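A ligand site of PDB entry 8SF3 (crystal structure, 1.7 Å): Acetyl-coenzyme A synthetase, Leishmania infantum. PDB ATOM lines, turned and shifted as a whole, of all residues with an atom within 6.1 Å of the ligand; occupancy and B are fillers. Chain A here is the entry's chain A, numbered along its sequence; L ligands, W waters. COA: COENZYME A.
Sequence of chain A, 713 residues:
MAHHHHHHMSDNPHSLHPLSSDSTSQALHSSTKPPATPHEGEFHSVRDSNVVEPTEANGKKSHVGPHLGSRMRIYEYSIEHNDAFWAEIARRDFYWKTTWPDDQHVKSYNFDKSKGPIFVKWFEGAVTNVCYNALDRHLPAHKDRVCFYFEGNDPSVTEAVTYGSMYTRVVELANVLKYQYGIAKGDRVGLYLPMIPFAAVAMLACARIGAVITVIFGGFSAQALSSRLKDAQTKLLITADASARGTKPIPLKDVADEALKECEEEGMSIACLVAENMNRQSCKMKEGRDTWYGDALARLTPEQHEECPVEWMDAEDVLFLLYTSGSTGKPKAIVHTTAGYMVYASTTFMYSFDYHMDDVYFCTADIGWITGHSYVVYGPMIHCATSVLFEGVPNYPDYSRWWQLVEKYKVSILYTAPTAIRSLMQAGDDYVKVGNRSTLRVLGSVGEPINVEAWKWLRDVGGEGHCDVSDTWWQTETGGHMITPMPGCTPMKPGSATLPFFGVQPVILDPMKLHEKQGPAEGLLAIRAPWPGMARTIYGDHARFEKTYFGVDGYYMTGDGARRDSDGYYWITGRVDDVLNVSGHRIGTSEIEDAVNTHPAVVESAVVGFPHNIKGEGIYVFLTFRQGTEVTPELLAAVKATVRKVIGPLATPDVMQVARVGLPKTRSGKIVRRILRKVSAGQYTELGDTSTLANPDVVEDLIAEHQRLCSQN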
ATOM      1  N   PRO A 194      10.612  21.613  17.017  1.00  0.00           N
ATOM      2  CA  PRO A 194      11.932  21.232  16.483  1.00  0.00           C
ATOM      3  C   PRO A 194      12.029  21.616  15.004  1.00  0.00           C
ATOM      4  O   PRO A 194      11.079  22.092  14.410  1.00  0.00           O
ATOM      5  CB  PRO A 194      11.931  19.722  16.657  1.00  0.00           C
ATOM      6  CG  PRO A 194      10.487  19.339  16.402  1.00  0.00           C
ATOM      7  CD  PRO A 194       9.626  20.531  16.833  1.00  0.00           C
ATOM      8  N   MET A 195      13.189  21.329  14.399  1.00  0.00           N
ATOM      9  CA  MET A 195      13.465  21.763  13.029  1.00  0.00           C
ATOM     10  C   MET A 195      12.949  20.667  12.116  1.00  0.00           C
ATOM     11  O   MET A 195      13.682  19.785  11.629  1.00  0.00           O
ATOM     12  CB  MET A 195      14.955  22.022  12.805  1.00  0.00           C
ATOM     13  CG  MET A 195      15.486  23.170  13.595  1.00  0.00           C
ATOM     14  SD  MET A 195      14.684  24.666  13.057  1.00  0.00           S
ATOM     15  CE  MET A 195      15.594  24.991  11.543  1.00  0.00           C
ATOM     16  N   PHE A 217      12.698  28.804  21.431  1.00  0.00           N
ATOM     17  CA  PHE A 217      13.686  27.770  21.150  1.00  0.00           C
ATOM     18  C   PHE A 217      13.404  26.503  21.954  1.00  0.00           C
ATOM     19  O   PHE A 217      13.131  26.566  23.152  1.00  0.00           O
ATOM     20  CB  PHE A 217      15.066  28.345  21.449  1.00  0.00           C
ATOM     21  CG  PHE A 217      16.195  27.356  21.484  1.00  0.00           C
ATOM     22  CD1 PHE A 217      16.570  26.660  20.330  1.00  0.00           C
ATOM     23  CD2 PHE A 217      16.920  27.174  22.637  1.00  0.00           C
ATOM     24  CE1 PHE A 217      17.647  25.797  20.355  1.00  0.00           C
ATOM     25  CE2 PHE A 217      18.000  26.298  22.668  1.00  0.00           C
ATOM     26  CZ  PHE A 217      18.357  25.611  21.524  1.00  0.00           C
ATOM     27  N   GLY A 218      13.463  25.361  21.277  1.00  0.00           N
ATOM     28  CA  GLY A 218      13.129  24.072  21.887  1.00  0.00           C
ATOM     29  C   GLY A 218      13.982  23.673  23.076  1.00  0.00           C
ATOM     30  O   GLY A 218      13.604  22.764  23.830  1.00  0.00           O
ATOM     31  N   GLY A 219      15.127  24.319  23.243  1.00  0.00           N
ATOM     32  CA  GLY A 219      15.980  24.073  24.390  1.00  0.00           C
ATOM     33  C   GLY A 219      15.611  24.838  25.649  1.00  0.00           C
ATOM     34  O   GLY A 219      16.187  24.575  26.714  1.00  0.00           O
ATOM     35  N   PHE A 220      14.670  25.791  25.571  1.00  0.00           N
ATOM     36  CA  PHE A 220      14.226  26.448  26.794  1.00  0.00           C
ATOM     37  C   PHE A 220      13.414  25.477  27.638  1.00  0.00           C
ATOM     38  O   PHE A 220      12.739  24.571  27.137  1.00  0.00           O
ATOM     39  CB  PHE A 220      13.390  27.698  26.482  1.00  0.00           C
ATOM     40  CG  PHE A 220      14.205  28.895  26.115  1.00  0.00           C
ATOM     41  CD1 PHE A 220      15.099  29.456  27.046  1.00  0.00           C
ATOM     42  CD2 PHE A 220      14.094  29.476  24.864  1.00  0.00           C
ATOM     43  CE1 PHE A 220      15.837  30.562  26.720  1.00  0.00           C
ATOM     44  CE2 PHE A 220      14.865  30.586  24.515  1.00  0.00           C
ATOM     45  CZ  PHE A 220      15.726  31.131  25.442  1.00  0.00           C
ATOM     46  N   ARG A 245      17.728  14.609  19.799  1.00  0.00           N
ATOM     47  CA  ARG A 245      18.967  15.284  19.403  1.00  0.00           C
ATOM     48  C   ARG A 245      20.103  14.379  19.800  1.00  0.00           C
ATOM     49  O   ARG A 245      20.413  14.258  20.992  1.00  0.00           O
ATOM     50  CB  ARG A 245      19.094  16.661  20.053  1.00  0.00           C
ATOM     51  CG  ARG A 245      18.484  17.801  19.231  1.00  0.00           C
ATOM     52  CD  ARG A 245      18.842  19.169  19.810  1.00  0.00           C
ATOM     53  NE  ARG A 245      20.202  19.625  19.486  1.00  0.00           N
ATOM     54  CZ  ARG A 245      20.508  20.312  18.387  1.00  0.00           C
ATOM     55  NH1 ARG A 245      19.609  20.509  17.423  1.00  0.00           N
ATOM     56  NH2 ARG A 245      21.726  20.822  18.255  1.00  0.00           N
ATOM     57  N   LYS A 248      19.714  12.018  22.862  1.00  0.00           N
ATOM     58  CA  LYS A 248      18.872  12.607  23.907  1.00  0.00           C
ATOM     59  C   LYS A 248      17.427  12.746  23.445  1.00  0.00           C
ATOM     60  O   LYS A 248      17.175  13.419  22.424  1.00  0.00           O
ATOM     61  CB  LYS A 248      19.423  13.982  24.321  1.00  0.00           C
ATOM     62  CG  LYS A 248      18.648  14.647  25.437  1.00  0.00           C
ATOM     63  CD  LYS A 248      19.163  16.058  25.788  1.00  0.00           C
ATOM     64  CE  LYS A 248      18.216  16.697  26.814  1.00  0.00           C
ATOM     65  NZ  LYS A 248      18.622  18.061  27.269  1.00  0.00           N
ATOM     66  N   ILE A 250      14.021  14.621  23.330  1.00  0.00           N
ATOM     67  CA  ILE A 250      13.623  16.007  23.562  1.00  0.00           C
ATOM     68  C   ILE A 250      12.120  16.019  23.806  1.00  0.00           C
ATOM     69  O   ILE A 250      11.328  16.031  22.853  1.00  0.00           O
ATOM     70  CB  ILE A 250      13.979  16.929  22.387  1.00  0.00           C
ATOM     71  CG1 ILE A 250      15.467  16.806  22.037  1.00  0.00           C
ATOM     72  CG2 ILE A 250      13.593  18.367  22.738  1.00  0.00           C
ATOM     73  CD1 ILE A 250      16.411  17.133  23.165  1.00  0.00           C
ATOM     74  N   LEU A 252       8.779  17.685  24.178  1.00  0.00           N
ATOM     75  CA  LEU A 252       8.261  18.998  23.834  1.00  0.00           C
ATOM     76  C   LEU A 252       6.887  19.182  24.460  1.00  0.00           C
ATOM     77  O   LEU A 252       6.725  20.056  25.291  1.00  0.00           O
ATOM     78  CB  LEU A 252       8.233  19.204  22.323  1.00  0.00           C
ATOM     79  CG  LEU A 252       9.607  19.287  21.664  1.00  0.00           C
ATOM     80  CD1 LEU A 252       9.489  19.218  20.172  1.00  0.00           C
ATOM     81  CD2 LEU A 252      10.332  20.580  22.079  1.00  0.00           C
ATOM     82  N   ASP A 366      18.785  27.246  14.293  1.00  0.00           N
ATOM     83  CA  ASP A 366      17.445  26.895  14.765  1.00  0.00           C
ATOM     84  C   ASP A 366      16.484  28.054  14.592  1.00  0.00           C
ATOM     85  O   ASP A 366      16.860  29.215  14.728  1.00  0.00           O
ATOM     86  CB  ASP A 366      17.508  26.486  16.239  1.00  0.00           C
ATOM     87  CG  ASP A 366      16.278  25.751  16.711  1.00  0.00           C
ATOM     88  OD1 ASP A 366      15.285  26.393  17.139  1.00  0.00           O
ATOM     89  OD2 ASP A 366      16.300  24.500  16.658  1.00  0.00           O
ATOM     90  N   VAL A 393      21.774  16.901  14.921  1.00  0.00           N
ATOM     91  CA  VAL A 393      22.999  17.493  15.460  1.00  0.00           C
ATOM     92  C   VAL A 393      24.170  17.013  14.614  1.00  0.00           C
ATOM     93  O   VAL A 393      24.101  15.926  14.031  1.00  0.00           O
ATOM     94  CB  VAL A 393      23.189  17.093  16.933  1.00  0.00           C
ATOM     95  CG1 VAL A 393      22.119  17.663  17.797  1.00  0.00           C
ATOM     96  CG2 VAL A 393      23.268  15.550  17.086  1.00  0.00           C
ATOM     97  N   PRO A 394      25.271  17.781  14.537  1.00  0.00           N
ATOM     98  CA  PRO A 394      26.377  17.400  13.641  1.00  0.00           C
ATOM     99  C   PRO A 394      27.140  16.158  14.043  1.00  0.00           C
ATOM    100  O   PRO A 394      27.966  15.695  13.248  1.00  0.00           O
ATOM    101  CB  PRO A 394      27.296  18.621  13.689  1.00  0.00           C
ATOM    102  CG  PRO A 394      26.938  19.333  14.946  1.00  0.00           C
ATOM    103  CD  PRO A 394      25.463  19.138  15.075  1.00  0.00           C
ATOM    104  N   ASN A 395      26.901  15.587  15.218  1.00  0.00           N
ATOM    105  CA  ASN A 395      27.691  14.431  15.642  1.00  0.00           C
ATOM    106  C   ASN A 395      26.837  13.176  15.819  1.00  0.00           C
ATOM    107  O   ASN A 395      27.231  12.273  16.545  1.00  0.00           O
ATOM    108  CB  ASN A 395      28.458  14.755  16.920  1.00  0.00           C
ATOM    109  CG  ASN A 395      27.570  14.831  18.136  1.00  0.00           C
ATOM    110  OD1 ASN A 395      26.431  15.283  18.054  1.00  0.00           O
ATOM    111  ND2 ASN A 395      28.095  14.376  19.273  1.00  0.00           N
ATOM    112  N   SER A 583      27.982  30.542  22.850  1.00  0.00           N
ATOM    113  CA  SER A 583      27.703  29.756  21.656  1.00  0.00           C
ATOM    114  C   SER A 583      26.875  30.566  20.653  1.00  0.00           C
ATOM    115  O   SER A 583      26.025  30.026  19.952  1.00  0.00           O
ATOM    116  CB  SER A 583      26.992  28.426  21.975  1.00  0.00           C
ATOM    117  OG  SER A 583      27.781  27.633  22.851  1.00  0.00           O
ATOM    118  N   LYS A 615      32.971  27.315  22.839  1.00  0.00           N
ATOM    119  CA  LYS A 615      31.779  28.168  22.878  1.00  0.00           C
ATOM    120  C   LYS A 615      32.082  29.645  22.709  1.00  0.00           C
ATOM    121  O   LYS A 615      31.138  30.439  22.661  1.00  0.00           O
ATOM    122  CB  LYS A 615      31.035  27.970  24.193  1.00  0.00           C
ATOM    123  CG  LYS A 615      30.912  26.525  24.613  1.00  0.00           C
ATOM    124  CD  LYS A 615      29.525  26.143  25.126  1.00  0.00           C
ATOM    125  CE  LYS A 615      29.385  26.321  26.624  1.00  0.00           C
ATOM    126  NZ  LYS A 615      28.210  25.550  27.153  1.00  0.00           N
ATOM    127  N   ARG A 644      19.221  24.922  34.855  1.00  0.00           N
ATOM    128  CA  ARG A 644      18.672  24.237  33.693  1.00  0.00           C
ATOM    129  C   ARG A 644      17.151  24.119  33.767  1.00  0.00           C
ATOM    130  O   ARG A 644      16.476  24.117  32.728  1.00  0.00           O
ATOM    131  CB  ARG A 644      19.341  22.875  33.557  1.00  0.00           C
ATOM    132  CG  ARG A 644      20.814  23.005  33.221  1.00  0.00           C
ATOM    133  CD  ARG A 644      21.561  21.679  33.263  1.00  0.00           C
ATOM    134  NE  ARG A 644      20.951  20.644  32.445  1.00  0.00           N
ATOM    135  CZ  ARG A 644      21.351  20.261  31.244  1.00  0.00           C
ATOM    136  NH1 ARG A 644      22.371  20.864  30.631  1.00  0.00           N
ATOM    137  NH2 ARG A 644      20.738  19.246  30.641  1.00  0.00           N
ATOM    138  N   PRO A 649      18.959  24.045  29.325  1.00  0.00           N
ATOM    139  CA  PRO A 649      20.315  23.560  29.103  1.00  0.00           C
ATOM    140  C   PRO A 649      21.260  24.573  28.498  1.00  0.00           C
ATOM    141  O   PRO A 649      22.465  24.550  28.791  1.00  0.00           O
ATOM    142  CB  PRO A 649      20.089  22.373  28.154  1.00  0.00           C
ATOM    143  CG  PRO A 649      18.763  21.882  28.508  1.00  0.00           C
ATOM    144  CD  PRO A 649      17.942  23.031  28.986  1.00  0.00           C
ATOM    145  N   LEU A 650      20.761  25.481  27.666  1.00  0.00           N
ATOM    146  CA  LEU A 650      21.652  26.459  27.057  1.00  0.00           C
ATOM    147  C   LEU A 650      22.367  27.304  28.079  1.00  0.00           C
ATOM    148  O   LEU A 650      23.425  27.855  27.785  1.00  0.00           O
ATOM    149  CB  LEU A 650      20.878  27.357  26.090  1.00  0.00           C
ATOM    150  CG  LEU A 650      19.905  28.393  26.664  1.00  0.00           C
ATOM    151  CD1 LEU A 650      19.391  29.352  25.572  1.00  0.00           C
ATOM    152  CD2 LEU A 650      18.718  27.732  27.366  1.00  0.00           C
ATOM    153  N   THR A 652      23.532  26.282  31.064  1.00  0.00           N
ATOM    154  CA  THR A 652      24.326  25.475  31.978  1.00  0.00           C
ATOM    155  C   THR A 652      25.659  26.162  32.305  1.00  0.00           C
ATOM    156  O   THR A 652      26.447  26.437  31.392  1.00  0.00           O
ATOM    157  CB  THR A 652      24.605  24.091  31.382  1.00  0.00           C
ATOM    158  OG1 THR A 652      23.364  23.450  31.048  1.00  0.00           O
ATOM    159  CG2 THR A 652      25.363  23.211  32.362  1.00  0.00           C
HETATM  160  N1A COA L   1      16.141  21.605  21.285  1.00  0.00           N
HETATM  161  C2A COA L   1      16.303  21.137  22.536  1.00  0.00           C
HETATM  162  N3A COA L   1      17.419  21.045  23.261  1.00  0.00           N
HETATM  163  C4A COA L   1      18.475  21.547  22.594  1.00  0.00           C
HETATM  164  C5A COA L   1      18.464  22.092  21.325  1.00  0.00           C
HETATM  165  C6A COA L   1      17.228  22.107  20.640  1.00  0.00           C
HETATM  166  N6A COA L   1      17.080  22.581  19.397  1.00  0.00           N
HETATM  167  N7A COA L   1      19.736  22.507  20.962  1.00  0.00           N
HETATM  168  C8A COA L   1      20.478  22.222  22.010  1.00  0.00           C
HETATM  169  N9A COA L   1      19.766  21.644  23.038  1.00  0.00           N
HETATM  170  C1B COA L   1      20.310  21.172  24.309  1.00  0.00           C
HETATM  171  C2B COA L   1      21.258  20.016  24.053  1.00  0.00           C
HETATM  172  O2B COA L   1      20.567  18.788  23.958  1.00  0.00           O
HETATM  173  C3B COA L   1      22.182  20.089  25.273  1.00  0.00           C
HETATM  174  O3B COA L   1      21.584  19.413  26.366  1.00  0.00           O
HETATM  175  P3B COA L   1      22.439  18.607  27.497  1.00  0.00           P
HETATM  176  O7A COA L   1      23.277  19.626  28.265  1.00  0.00           O
HETATM  177  O8A COA L   1      21.327  17.942  28.282  1.00  0.00           O
HETATM  178  O9A COA L   1      23.342  17.591  26.798  1.00  0.00           O
HETATM  179  C4B COA L   1      22.243  21.589  25.563  1.00  0.00           C
HETATM  180  O4B COA L   1      21.136  22.187  24.850  1.00  0.00           O
HETATM  181  C5B COA L   1      23.509  22.243  25.068  1.00  0.00           C
HETATM  182  O5B COA L   1      23.599  21.998  23.654  1.00  0.00           O
HETATM  183  P1A COA L   1      25.094  21.913  23.075  1.00  0.00           P
HETATM  184  O1A COA L   1      25.703  20.607  23.432  1.00  0.00           O
HETATM  185  O2A COA L   1      25.781  23.182  23.417  1.00  0.00           O
HETATM  186  O3A COA L   1      24.786  21.868  21.508  1.00  0.00           O
HETATM  187  P2A COA L   1      24.527  20.613  20.522  1.00  0.00           P
HETATM  188  O4A COA L   1      25.821  19.808  20.530  1.00  0.00           O
HETATM  189  O5A COA L   1      23.374  19.840  21.109  1.00  0.00           O
HETATM  190  O6A COA L   1      24.216  21.246  19.177  1.00  0.00           O
HETATM  191  O   HOH W   1      14.017  20.938  19.618  1.00  0.00           O
HETATM  192  O   HOH W   2      17.085  20.021  25.716  1.00  0.00           O
HETATM  193  O   HOH W   3      21.247  15.597  29.156  1.00  0.00           O
HETATM  194  O   HOH W   4      14.932  22.480  17.550  1.00  0.00           O
HETATM  195  O   HOH W   5      20.129  23.966  18.586  1.00  0.00           O
HETATM  196  O   HOH W   6      25.032  23.530  27.627  1.00  0.00           O
HETATM  197  O   HOH W   7      22.973  15.641  25.126  1.00  0.00           O
HETATM  198  O   HOH W   8      21.765  16.445  22.679  1.00  0.00           O
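O of Pro 649 lies within hydrogen-bond range of OG1 of Thr 652 (2.7 Å).
The side-chain hydroxyl of Thr 652 sits at hydrogen-bond distance from the guanidinium group of Arg 644 (2.8 Å).
Water W2 bridges a nitrogen (N3A) of the ligand (2.7 Å) and the side-chain amino group of Lys 248 (2.9 Å).
Water W4 bridges OD2 of Asp 366 (2.6 Å) and N6A of the ligand (2.8 Å).
Water W8 bridges an oxygen (O2B) of the ligand (2.9 Å) and the backbone carbonyl oxygen (O) of Arg 245 (3.1 Å).
Merely in contact with the ligand: Phe 217 (3.4 Å), Gly 218 (3.4 Å), Ile 250 (3.9 Å) and Pro 649 (3.5 Å).
Nine residues have an atom within 4 Å of the ligand: Phe 217, Gly 218, Gly 219, Arg 245, Lys 248, Ile 250, Asp 366, Arg 644 and Pro 649.
The nearest printed residue that does not touch the ligand is Val 393 (4.2 Å).
The backbone NH (N) of Gly 219 sits close to a nitrogen (N1A) of the ligand.
An oxygen (O8A) of the ligand is in salt-bridge range of the side-chain amino group (NZ) of Lys 248 (2.9 Å).
OD2 of Asp 366 lies within hydrogen-bond range of N6A of the ligand, 3.4 Å away.
NH2 of Arg 245 is in salt-bridge range of O6A of the ligand (2.7 Å).
NH2 of Arg 644 lies within salt-bridge range of O8A of the ligand (2.8 Å).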
